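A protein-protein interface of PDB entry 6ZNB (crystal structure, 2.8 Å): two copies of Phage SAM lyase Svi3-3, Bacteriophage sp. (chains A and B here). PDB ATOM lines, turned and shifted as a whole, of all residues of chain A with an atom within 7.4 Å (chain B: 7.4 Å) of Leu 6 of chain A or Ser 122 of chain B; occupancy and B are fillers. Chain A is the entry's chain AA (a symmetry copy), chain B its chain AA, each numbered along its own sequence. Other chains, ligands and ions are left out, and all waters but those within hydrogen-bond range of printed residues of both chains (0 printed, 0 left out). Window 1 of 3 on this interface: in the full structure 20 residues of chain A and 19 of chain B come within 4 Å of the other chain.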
ATOM      1  N   SER A   1      -7.869   0.422 -11.815  1.00  0.00           N
ATOM      2  CA  SER A   1      -7.589   0.690 -13.217  1.00  0.00           C
ATOM      3  C   SER A   1      -8.296  -0.331 -14.100  1.00  0.00           C
ATOM      4  O   SER A   1      -8.187  -1.524 -13.883  1.00  0.00           O
ATOM      5  CB  SER A   1      -6.084   0.672 -13.492  1.00  0.00           C
ATOM      6  OG  SER A   1      -5.747  -0.644 -13.850  1.00  0.00           O
ATOM      7  N   LEU A   2      -9.027   0.152 -15.096  1.00  0.00           N
ATOM      8  CA  LEU A   2      -9.758  -0.716 -16.010  1.00  0.00           C
ATOM      9  C   LEU A   2      -8.941  -0.887 -17.284  1.00  0.00           C
ATOM     10  O   LEU A   2      -8.593   0.101 -17.939  1.00  0.00           O
ATOM     11  CB  LEU A   2     -11.133  -0.125 -16.315  1.00  0.00           C
ATOM     12  CG  LEU A   2     -11.940  -0.681 -17.486  1.00  0.00           C
ATOM     13  CD1 LEU A   2     -12.201  -2.167 -17.304  1.00  0.00           C
ATOM     14  CD2 LEU A   2     -13.237   0.095 -17.572  1.00  0.00           C
ATOM     15  N   MET A   3      -8.615  -2.138 -17.622  1.00  0.00           N
ATOM     16  CA  MET A   3      -7.824  -2.463 -18.809  1.00  0.00           C
ATOM     17  C   MET A   3      -8.756  -2.998 -19.890  1.00  0.00           C
ATOM     18  O   MET A   3      -9.317  -4.090 -19.750  1.00  0.00           O
ATOM     19  CB  MET A   3      -6.728  -3.477 -18.483  1.00  0.00           C
ATOM     20  CG  MET A   3      -5.716  -3.666 -19.602  1.00  0.00           C
ATOM     21  SD  MET A   3      -4.327  -4.701 -19.110  1.00  0.00           S
ATOM     22  CE  MET A   3      -3.723  -3.794 -17.689  1.00  0.00           C
ATOM     23  N   GLU A   4      -8.909  -2.235 -20.971  1.00  0.00           N
ATOM     24  CA  GLU A   4      -9.797  -2.588 -22.069  1.00  0.00           C
ATOM     25  C   GLU A   4      -8.989  -2.707 -23.354  1.00  0.00           C
ATOM     26  O   GLU A   4      -8.183  -1.826 -23.674  1.00  0.00           O
ATOM     27  CB  GLU A   4     -10.924  -1.553 -22.215  1.00  0.00           C
ATOM     28  CG  GLU A   4     -10.469  -0.144 -22.579  1.00  0.00           C
ATOM     29  CD  GLU A   4     -11.388   0.949 -22.060  1.00  0.00           C
ATOM     30  OE1 GLU A   4     -10.997   1.635 -21.093  1.00  0.00           O
ATOM     31  OE2 GLU A   4     -12.486   1.133 -22.627  1.00  0.00           O
ATOM     32  N   ARG A   5      -9.186  -3.809 -24.071  1.00  0.00           N
ATOM     33  CA  ARG A   5      -8.520  -4.028 -25.350  1.00  0.00           C
ATOM     34  C   ARG A   5      -9.302  -3.299 -26.434  1.00  0.00           C
ATOM     35  O   ARG A   5     -10.392  -3.732 -26.821  1.00  0.00           O
ATOM     36  CB  ARG A   5      -8.417  -5.520 -25.652  1.00  0.00           C
ATOM     37  CG  ARG A   5      -7.404  -5.886 -26.729  1.00  0.00           C
ATOM     38  CD  ARG A   5      -7.387  -7.389 -26.966  1.00  0.00           C
ATOM     39  NE  ARG A   5      -6.587  -7.767 -28.128  1.00  0.00           N
ATOM     40  CZ  ARG A   5      -7.033  -7.749 -29.380  1.00  0.00           C
ATOM     41  NH1 ARG A   5      -8.277  -7.370 -29.639  1.00  0.00           N
ATOM     42  NH2 ARG A   5      -6.235  -8.110 -30.375  1.00  0.00           N
ATOM     43  N   LEU A   6      -8.750  -2.188 -26.927  1.00  0.00           N
ATOM     44  CA  LEU A   6      -9.466  -1.396 -27.922  1.00  0.00           C
ATOM     45  C   LEU A   6      -9.560  -2.115 -29.261  1.00  0.00           C
ATOM     46  O   LEU A   6     -10.492  -1.861 -30.033  1.00  0.00           O
ATOM     47  CB  LEU A   6      -8.799  -0.032 -28.089  1.00  0.00           C
ATOM     48  CG  LEU A   6      -8.429   0.696 -26.794  1.00  0.00           C
ATOM     49  CD1 LEU A   6      -7.716   2.002 -27.101  1.00  0.00           C
ATOM     50  CD2 LEU A   6      -9.674   0.946 -25.957  1.00  0.00           C
ATOM     51  N   GLY A   7      -8.628  -3.012 -29.553  1.00  0.00           N
ATOM     52  CA  GLY A   7      -8.676  -3.754 -30.798  1.00  0.00           C
ATOM     53  C   GLY A   7      -7.294  -4.264 -31.169  1.00  0.00           C
ATOM     54  O   GLY A   7      -6.387  -4.298 -30.341  1.00  0.00           O
ATOM     55  N   GLY A   8      -7.169  -4.659 -32.437  1.00  0.00           N
ATOM     56  CA  GLY A   8      -5.925  -5.190 -32.952  1.00  0.00           C
ATOM     57  C   GLY A   8      -5.013  -4.191 -33.624  1.00  0.00           C
ATOM     58  O   GLY A   8      -3.911  -4.559 -34.042  1.00  0.00           O
ATOM     59  N   GLY A   9      -5.435  -2.935 -33.743  1.00  0.00           N
ATOM     60  CA  GLY A   9      -4.610  -1.926 -34.375  1.00  0.00           C
ATOM     61  C   GLY A   9      -5.367  -0.668 -34.750  1.00  0.00           C
ATOM     62  O   GLY A   9      -5.479   0.261 -33.944  1.00  0.00           O
ATOM     63  N   LEU A  79      -9.043   8.097 -34.084  1.00  0.00           N
ATOM     64  CA  LEU A  79      -9.832   8.032 -32.858  1.00  0.00           C
ATOM     65  C   LEU A  79     -11.324   8.195 -33.120  1.00  0.00           C
ATOM     66  O   LEU A  79     -12.143   7.558 -32.448  1.00  0.00           O
ATOM     67  CB  LEU A  79      -9.367   9.110 -31.877  1.00  0.00           C
ATOM     68  CG  LEU A  79      -7.895   9.074 -31.461  1.00  0.00           C
ATOM     69  CD1 LEU A  79      -7.577  10.205 -30.491  1.00  0.00           C
ATOM     70  CD2 LEU A  79      -7.552   7.726 -30.854  1.00  0.00           C
ATOM     71  N   GLN B  92       1.665  -4.919 -19.530  1.00  0.00           N
ATOM     72  CA  GLN B  92       0.427  -4.386 -18.974  1.00  0.00           C
ATOM     73  C   GLN B  92       0.569  -4.083 -17.489  1.00  0.00           C
ATOM     74  O   GLN B  92      -0.024  -3.118 -16.995  1.00  0.00           O
ATOM     75  CB  GLN B  92      -0.719  -5.368 -19.217  1.00  0.00           C
ATOM     76  CG  GLN B  92      -1.059  -5.559 -20.688  1.00  0.00           C
ATOM     77  CD  GLN B  92      -2.168  -6.567 -20.908  1.00  0.00           C
ATOM     78  OE1 GLN B  92      -1.946  -7.776 -20.846  1.00  0.00           O
ATOM     79  NE2 GLN B  92      -3.371  -6.073 -21.178  1.00  0.00           N
ATOM     80  N   GLU B 105      -4.599   9.798 -15.918  1.00  0.00           N
ATOM     81  CA  GLU B 105      -5.970   9.348 -16.124  1.00  0.00           C
ATOM     82  C   GLU B 105      -6.015   8.128 -17.032  1.00  0.00           C
ATOM     83  O   GLU B 105      -6.900   7.276 -16.884  1.00  0.00           O
ATOM     84  CB  GLU B 105      -6.811  10.483 -16.708  1.00  0.00           C
ATOM     85  CG  GLU B 105      -8.257  10.109 -16.998  1.00  0.00           C
ATOM     86  CD  GLU B 105      -9.014  11.211 -17.710  1.00  0.00           C
ATOM     87  OE1 GLU B 105      -8.363  12.066 -18.349  1.00  0.00           O
ATOM     88  OE2 GLU B 105     -10.261  11.224 -17.632  1.00  0.00           O
ATOM     89  N   SER B 106      -5.067   8.018 -17.962  1.00  0.00           N
ATOM     90  CA  SER B 106      -5.031   6.905 -18.896  1.00  0.00           C
ATOM     91  C   SER B 106      -3.596   6.655 -19.329  1.00  0.00           C
ATOM     92  O   SER B 106      -2.748   7.551 -19.298  1.00  0.00           O
ATOM     93  CB  SER B 106      -5.915   7.170 -20.121  1.00  0.00           C
ATOM     94  OG  SER B 106      -5.166   7.768 -21.166  1.00  0.00           O
ATOM     95  N   VAL B 107      -3.333   5.415 -19.735  1.00  0.00           N
ATOM     96  CA  VAL B 107      -2.051   5.012 -20.300  1.00  0.00           C
ATOM     97  C   VAL B 107      -2.327   4.010 -21.412  1.00  0.00           C
ATOM     98  O   VAL B 107      -3.080   3.050 -21.214  1.00  0.00           O
ATOM     99  CB  VAL B 107      -1.110   4.405 -19.238  1.00  0.00           C
ATOM    100  CG1 VAL B 107      -0.113   3.454 -19.880  1.00  0.00           C
ATOM    101  CG2 VAL B 107      -0.379   5.507 -18.486  1.00  0.00           C
ATOM    102  N   ILE B 108      -1.736   4.239 -22.581  1.00  0.00           N
ATOM    103  CA  ILE B 108      -1.912   3.357 -23.728  1.00  0.00           C
ATOM    104  C   ILE B 108      -0.779   2.342 -23.755  1.00  0.00           C
ATOM    105  O   ILE B 108       0.391   2.684 -23.542  1.00  0.00           O
ATOM    106  CB  ILE B 108      -1.970   4.165 -25.039  1.00  0.00           C
ATOM    107  CG1 ILE B 108      -3.168   5.112 -25.025  1.00  0.00           C
ATOM    108  CG2 ILE B 108      -2.053   3.234 -26.238  1.00  0.00           C
ATOM    109  CD1 ILE B 108      -4.501   4.399 -25.021  1.00  0.00           C
ATOM    110  N   VAL B 109      -1.130   1.083 -24.006  1.00  0.00           N
ATOM    111  CA  VAL B 109      -0.169  -0.002 -24.157  1.00  0.00           C
ATOM    112  C   VAL B 109      -0.443  -0.689 -25.485  1.00  0.00           C
ATOM    113  O   VAL B 109      -1.582  -1.082 -25.761  1.00  0.00           O
ATOM    114  CB  VAL B 109      -0.250  -1.010 -22.996  1.00  0.00           C
ATOM    115  CG1 VAL B 109       0.692  -2.172 -23.241  1.00  0.00           C
ATOM    116  CG2 VAL B 109       0.076  -0.324 -21.680  1.00  0.00           C
ATOM    117  N   GLU B 110       0.596  -0.835 -26.303  1.00  0.00           N
ATOM    118  CA  GLU B 110       0.465  -1.369 -27.653  1.00  0.00           C
ATOM    119  C   GLU B 110       1.496  -2.469 -27.851  1.00  0.00           C
ATOM    120  O   GLU B 110       2.702  -2.207 -27.805  1.00  0.00           O
ATOM    121  CB  GLU B 110       0.637  -0.257 -28.693  1.00  0.00           C
ATOM    122  CG  GLU B 110       1.013  -0.721 -30.087  1.00  0.00           C
ATOM    123  CD  GLU B 110       1.421   0.438 -30.977  1.00  0.00           C
ATOM    124  OE1 GLU B 110       1.039   1.587 -30.669  1.00  0.00           O
ATOM    125  OE2 GLU B 110       2.129   0.204 -31.980  1.00  0.00           O
ATOM    126  N   ASP B 119      -2.123  -6.012 -30.332  1.00  0.00           N
ATOM    127  CA  ASP B 119      -3.161  -5.484 -29.459  1.00  0.00           C
ATOM    128  C   ASP B 119      -2.783  -4.077 -29.032  1.00  0.00           C
ATOM    129  O   ASP B 119      -1.601  -3.720 -28.991  1.00  0.00           O
ATOM    130  CB  ASP B 119      -3.366  -6.360 -28.214  1.00  0.00           C
ATOM    131  CG  ASP B 119      -3.195  -7.838 -28.500  1.00  0.00           C
ATOM    132  OD1 ASP B 119      -4.099  -8.436 -29.123  1.00  0.00           O
ATOM    133  OD2 ASP B 119      -2.152  -8.402 -28.102  1.00  0.00           O
ATOM    134  N   VAL B 120      -3.799  -3.277 -28.716  1.00  0.00           N
ATOM    135  CA  VAL B 120      -3.621  -1.957 -28.122  1.00  0.00           C
ATOM    136  C   VAL B 120      -4.550  -1.888 -26.922  1.00  0.00           C
ATOM    137  O   VAL B 120      -5.775  -1.790 -27.084  1.00  0.00           O
ATOM    138  CB  VAL B 120      -3.915  -0.816 -29.104  1.00  0.00           C
ATOM    139  CG1 VAL B 120      -3.757   0.527 -28.410  1.00  0.00           C
ATOM    140  CG2 VAL B 120      -2.998  -0.896 -30.306  1.00  0.00           C
ATOM    141  N   TYR B 121      -3.981  -1.935 -25.724  1.00  0.00           N
ATOM    142  CA  TYR B 121      -4.754  -1.932 -24.495  1.00  0.00           C
ATOM    143  C   TYR B 121      -4.858  -0.520 -23.935  1.00  0.00           C
ATOM    144  O   TYR B 121      -3.916   0.272 -24.035  1.00  0.00           O
ATOM    145  CB  TYR B 121      -4.123  -2.858 -23.455  1.00  0.00           C
ATOM    146  CG  TYR B 121      -4.267  -4.329 -23.776  1.00  0.00           C
ATOM    147  CD1 TYR B 121      -5.418  -5.025 -23.431  1.00  0.00           C
ATOM    148  CD2 TYR B 121      -3.257  -5.018 -24.434  1.00  0.00           C
ATOM    149  CE1 TYR B 121      -5.555  -6.366 -23.723  1.00  0.00           C
ATOM    150  CE2 TYR B 121      -3.385  -6.360 -24.732  1.00  0.00           C
ATOM    151  CZ  TYR B 121      -4.537  -7.029 -24.376  1.00  0.00           C
ATOM    152  OH  TYR B 121      -4.669  -8.366 -24.672  1.00  0.00           O
ATOM    153  N   SER B 122      -6.012  -0.213 -23.354  1.00  0.00           N
ATOM    154  CA  SER B 122      -6.244   1.046 -22.664  1.00  0.00           C
ATOM    155  C   SER B 122      -6.245   0.803 -21.163  1.00  0.00           C
ATOM    156  O   SER B 122      -7.005  -0.039 -20.664  1.00  0.00           O
ATOM    157  CB  SER B 122      -7.568   1.684 -23.089  1.00  0.00           C
ATOM    158  OG  SER B 122      -7.765   2.921 -22.433  1.00  0.00           O
ATOM    159  N   ILE B 123      -5.404   1.546 -20.448  1.00  0.00           N
ATOM    160  CA  ILE B 123      -5.300   1.454 -18.994  1.00  0.00           C
ATOM    161  C   ILE B 123      -5.848   2.761 -18.434  1.00  0.00           C
ATOM    162  O   ILE B 123      -5.169   3.793 -18.461  1.00  0.00           O
ATOM    163  CB  ILE B 123      -3.862   1.193 -18.531  1.00  0.00           C
ATOM    164  CG1 ILE B 123      -3.386  -0.167 -19.048  1.00  0.00           C
ATOM    165  CG2 ILE B 123      -3.740   1.280 -17.023  1.00  0.00           C
ATOM    166  CD1 ILE B 123      -1.955  -0.488 -18.685  1.00  0.00           C
ATOM    167  N   THR B 124      -7.085   2.723 -17.943  1.00  0.00           N
ATOM    168  CA  THR B 124      -7.800   3.915 -17.514  1.00  0.00           C
ATOM    169  C   THR B 124      -8.074   3.856 -16.019  1.00  0.00           C
ATOM    170  O   THR B 124      -8.455   2.808 -15.489  1.00  0.00           O
ATOM    171  CB  THR B 124      -9.123   4.067 -18.271  1.00  0.00           C
ATOM    172  OG1 THR B 124      -8.956   3.620 -19.622  1.00  0.00           O
ATOM    173  CG2 THR B 124      -9.569   5.520 -18.270  1.00  0.00           C
ATOM    174  N   ALA B 125      -7.891   4.990 -15.350  1.00  0.00           N
ATOM    175  CA  ALA B 125      -8.166   5.084 -13.925  1.00  0.00           C
ATOM    176  C   ALA B 125      -9.666   5.158 -13.675  1.00  0.00           C
ATOM    177  O   ALA B 125     -10.397   5.854 -14.386  1.00  0.00           O
ATOM    178  CB  ALA B 125      -7.477   6.311 -13.326  1.00  0.00           C
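The side-chain sulfur (SD) of Met 3 of chain A lies within hydrogen-bond range of the side-chain amide nitrogen (NE2) of Gln 92 of chain B, at 2.7 Å. OD1 of Asp 119 of chain B lies within salt-bridge range of NH2 of Arg 5 of chain A, at 2.5 Å. N of Leu 6 of chain A lies within hydrogen-bond range of O of Val 120 of chain B (3.0 Å). The backbone NH (N) of Val 120 of chain B is in hydrogen-bond range of the backbone carbonyl oxygen (O) of Gly 7 of chain A. O of Glu 4 of chain A sits at hydrogen-bond distance from N of Ser 122 of chain B. The backbone NH of Leu 2 of chain A lies within hydrogen-bond range of the backbone carbonyl oxygen of Thr 124 of chain B (2.7 Å). The side-chain carboxylate (OE1) of Glu 4 of chain A is in hydrogen-bond range of the side-chain hydroxyl (OG1) of Thr 124 of chain B. The backbone carbonyl oxygen of Leu 2 of chain A lies close to the backbone carbonyl oxygen of Ser 122 of chain B, 3.2 Å away.
N of Val 107 of chain B lies within hydrogen-bond range of O of Ile 123 of chain B (2.8 Å). O of Val 109 of chain B is in hydrogen-bond range of N of Tyr 121 of chain B (2.5 Å). The side-chain hydroxyl of Ser 122 of chain B sits at hydrogen-bond distance from the side-chain hydroxyl of Thr 124 of chain B, at 3.1 Å.
No position is printed for both chains. Of the 17 pairs that touch across the chains among the printed residues, none has its exchanged pair printed and touching as well.
Among the printed residues, merely in contact across the chains: Met 3 of chain A with Ser 122 of chain B, Ser 1 of chain A with Thr 124 of chain B, Glu 4 of chain A with Tyr 121 of chain B, Gly 7 of chain A with Asp 119 of chain B, Arg 5 of chain A with Tyr 121 of chain B, Leu 6 of chain A with Ser 122 of chain B, Leu 2 of chain A with Ile 123 of chain B, Met 3 of chain A with Ile 123 of chain B and Arg 5 of chain A with Val 120 of chain B.
Printed residues of chain B within 4 Å of Ser 1 of chain A: Thr 124 (3.2 Å). Printed residues of chain B within 4 Å of Leu 2 of chain A: Ser 122, Ile 123 and Thr 124. Printed residues of chain B within 4 Å of Met 3 of chain A: Gln 92 (2.7 Å), Ser 122 (3.2 Å) and Ile 123 (3.9 Å). Of the printed residues of chain B, Arg 5 of chain A touches Asp 119 (2.5 Å), Val 120 (3.9 Å) and Tyr 121 (3.6 Å). Leu 6 of chain A touches two residues of chain B. Printed residues of chain A within 4 Å of Gln 92 of chain B: Met 3. Ser 122 of chain B touches four residues of chain A. The nearest residue of chain A that does not touch Ser 122 of chain B is Arg 5 of chain A (4.8 Å). The nearest printed residue of chain B that does not touch Leu 2 of chain A is Ala 125 of chain B (5.0 Å).
Along chain B the printed residues that touch a printed residue of chain A span positions 92 to 124. Hydrophobic or aromatic side chains of chain A that line the printed part of chain B: Met 3 and Leu 6. Among the printed residues, 17 pairs touch across the chains. Among the printed residues, Asp or Glu carboxylates within 4 Å of a Lys or Arg side-chain nitrogen of the other chain: Arg 5 of chain A with Asp 119 of chain B (2.5 Å).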
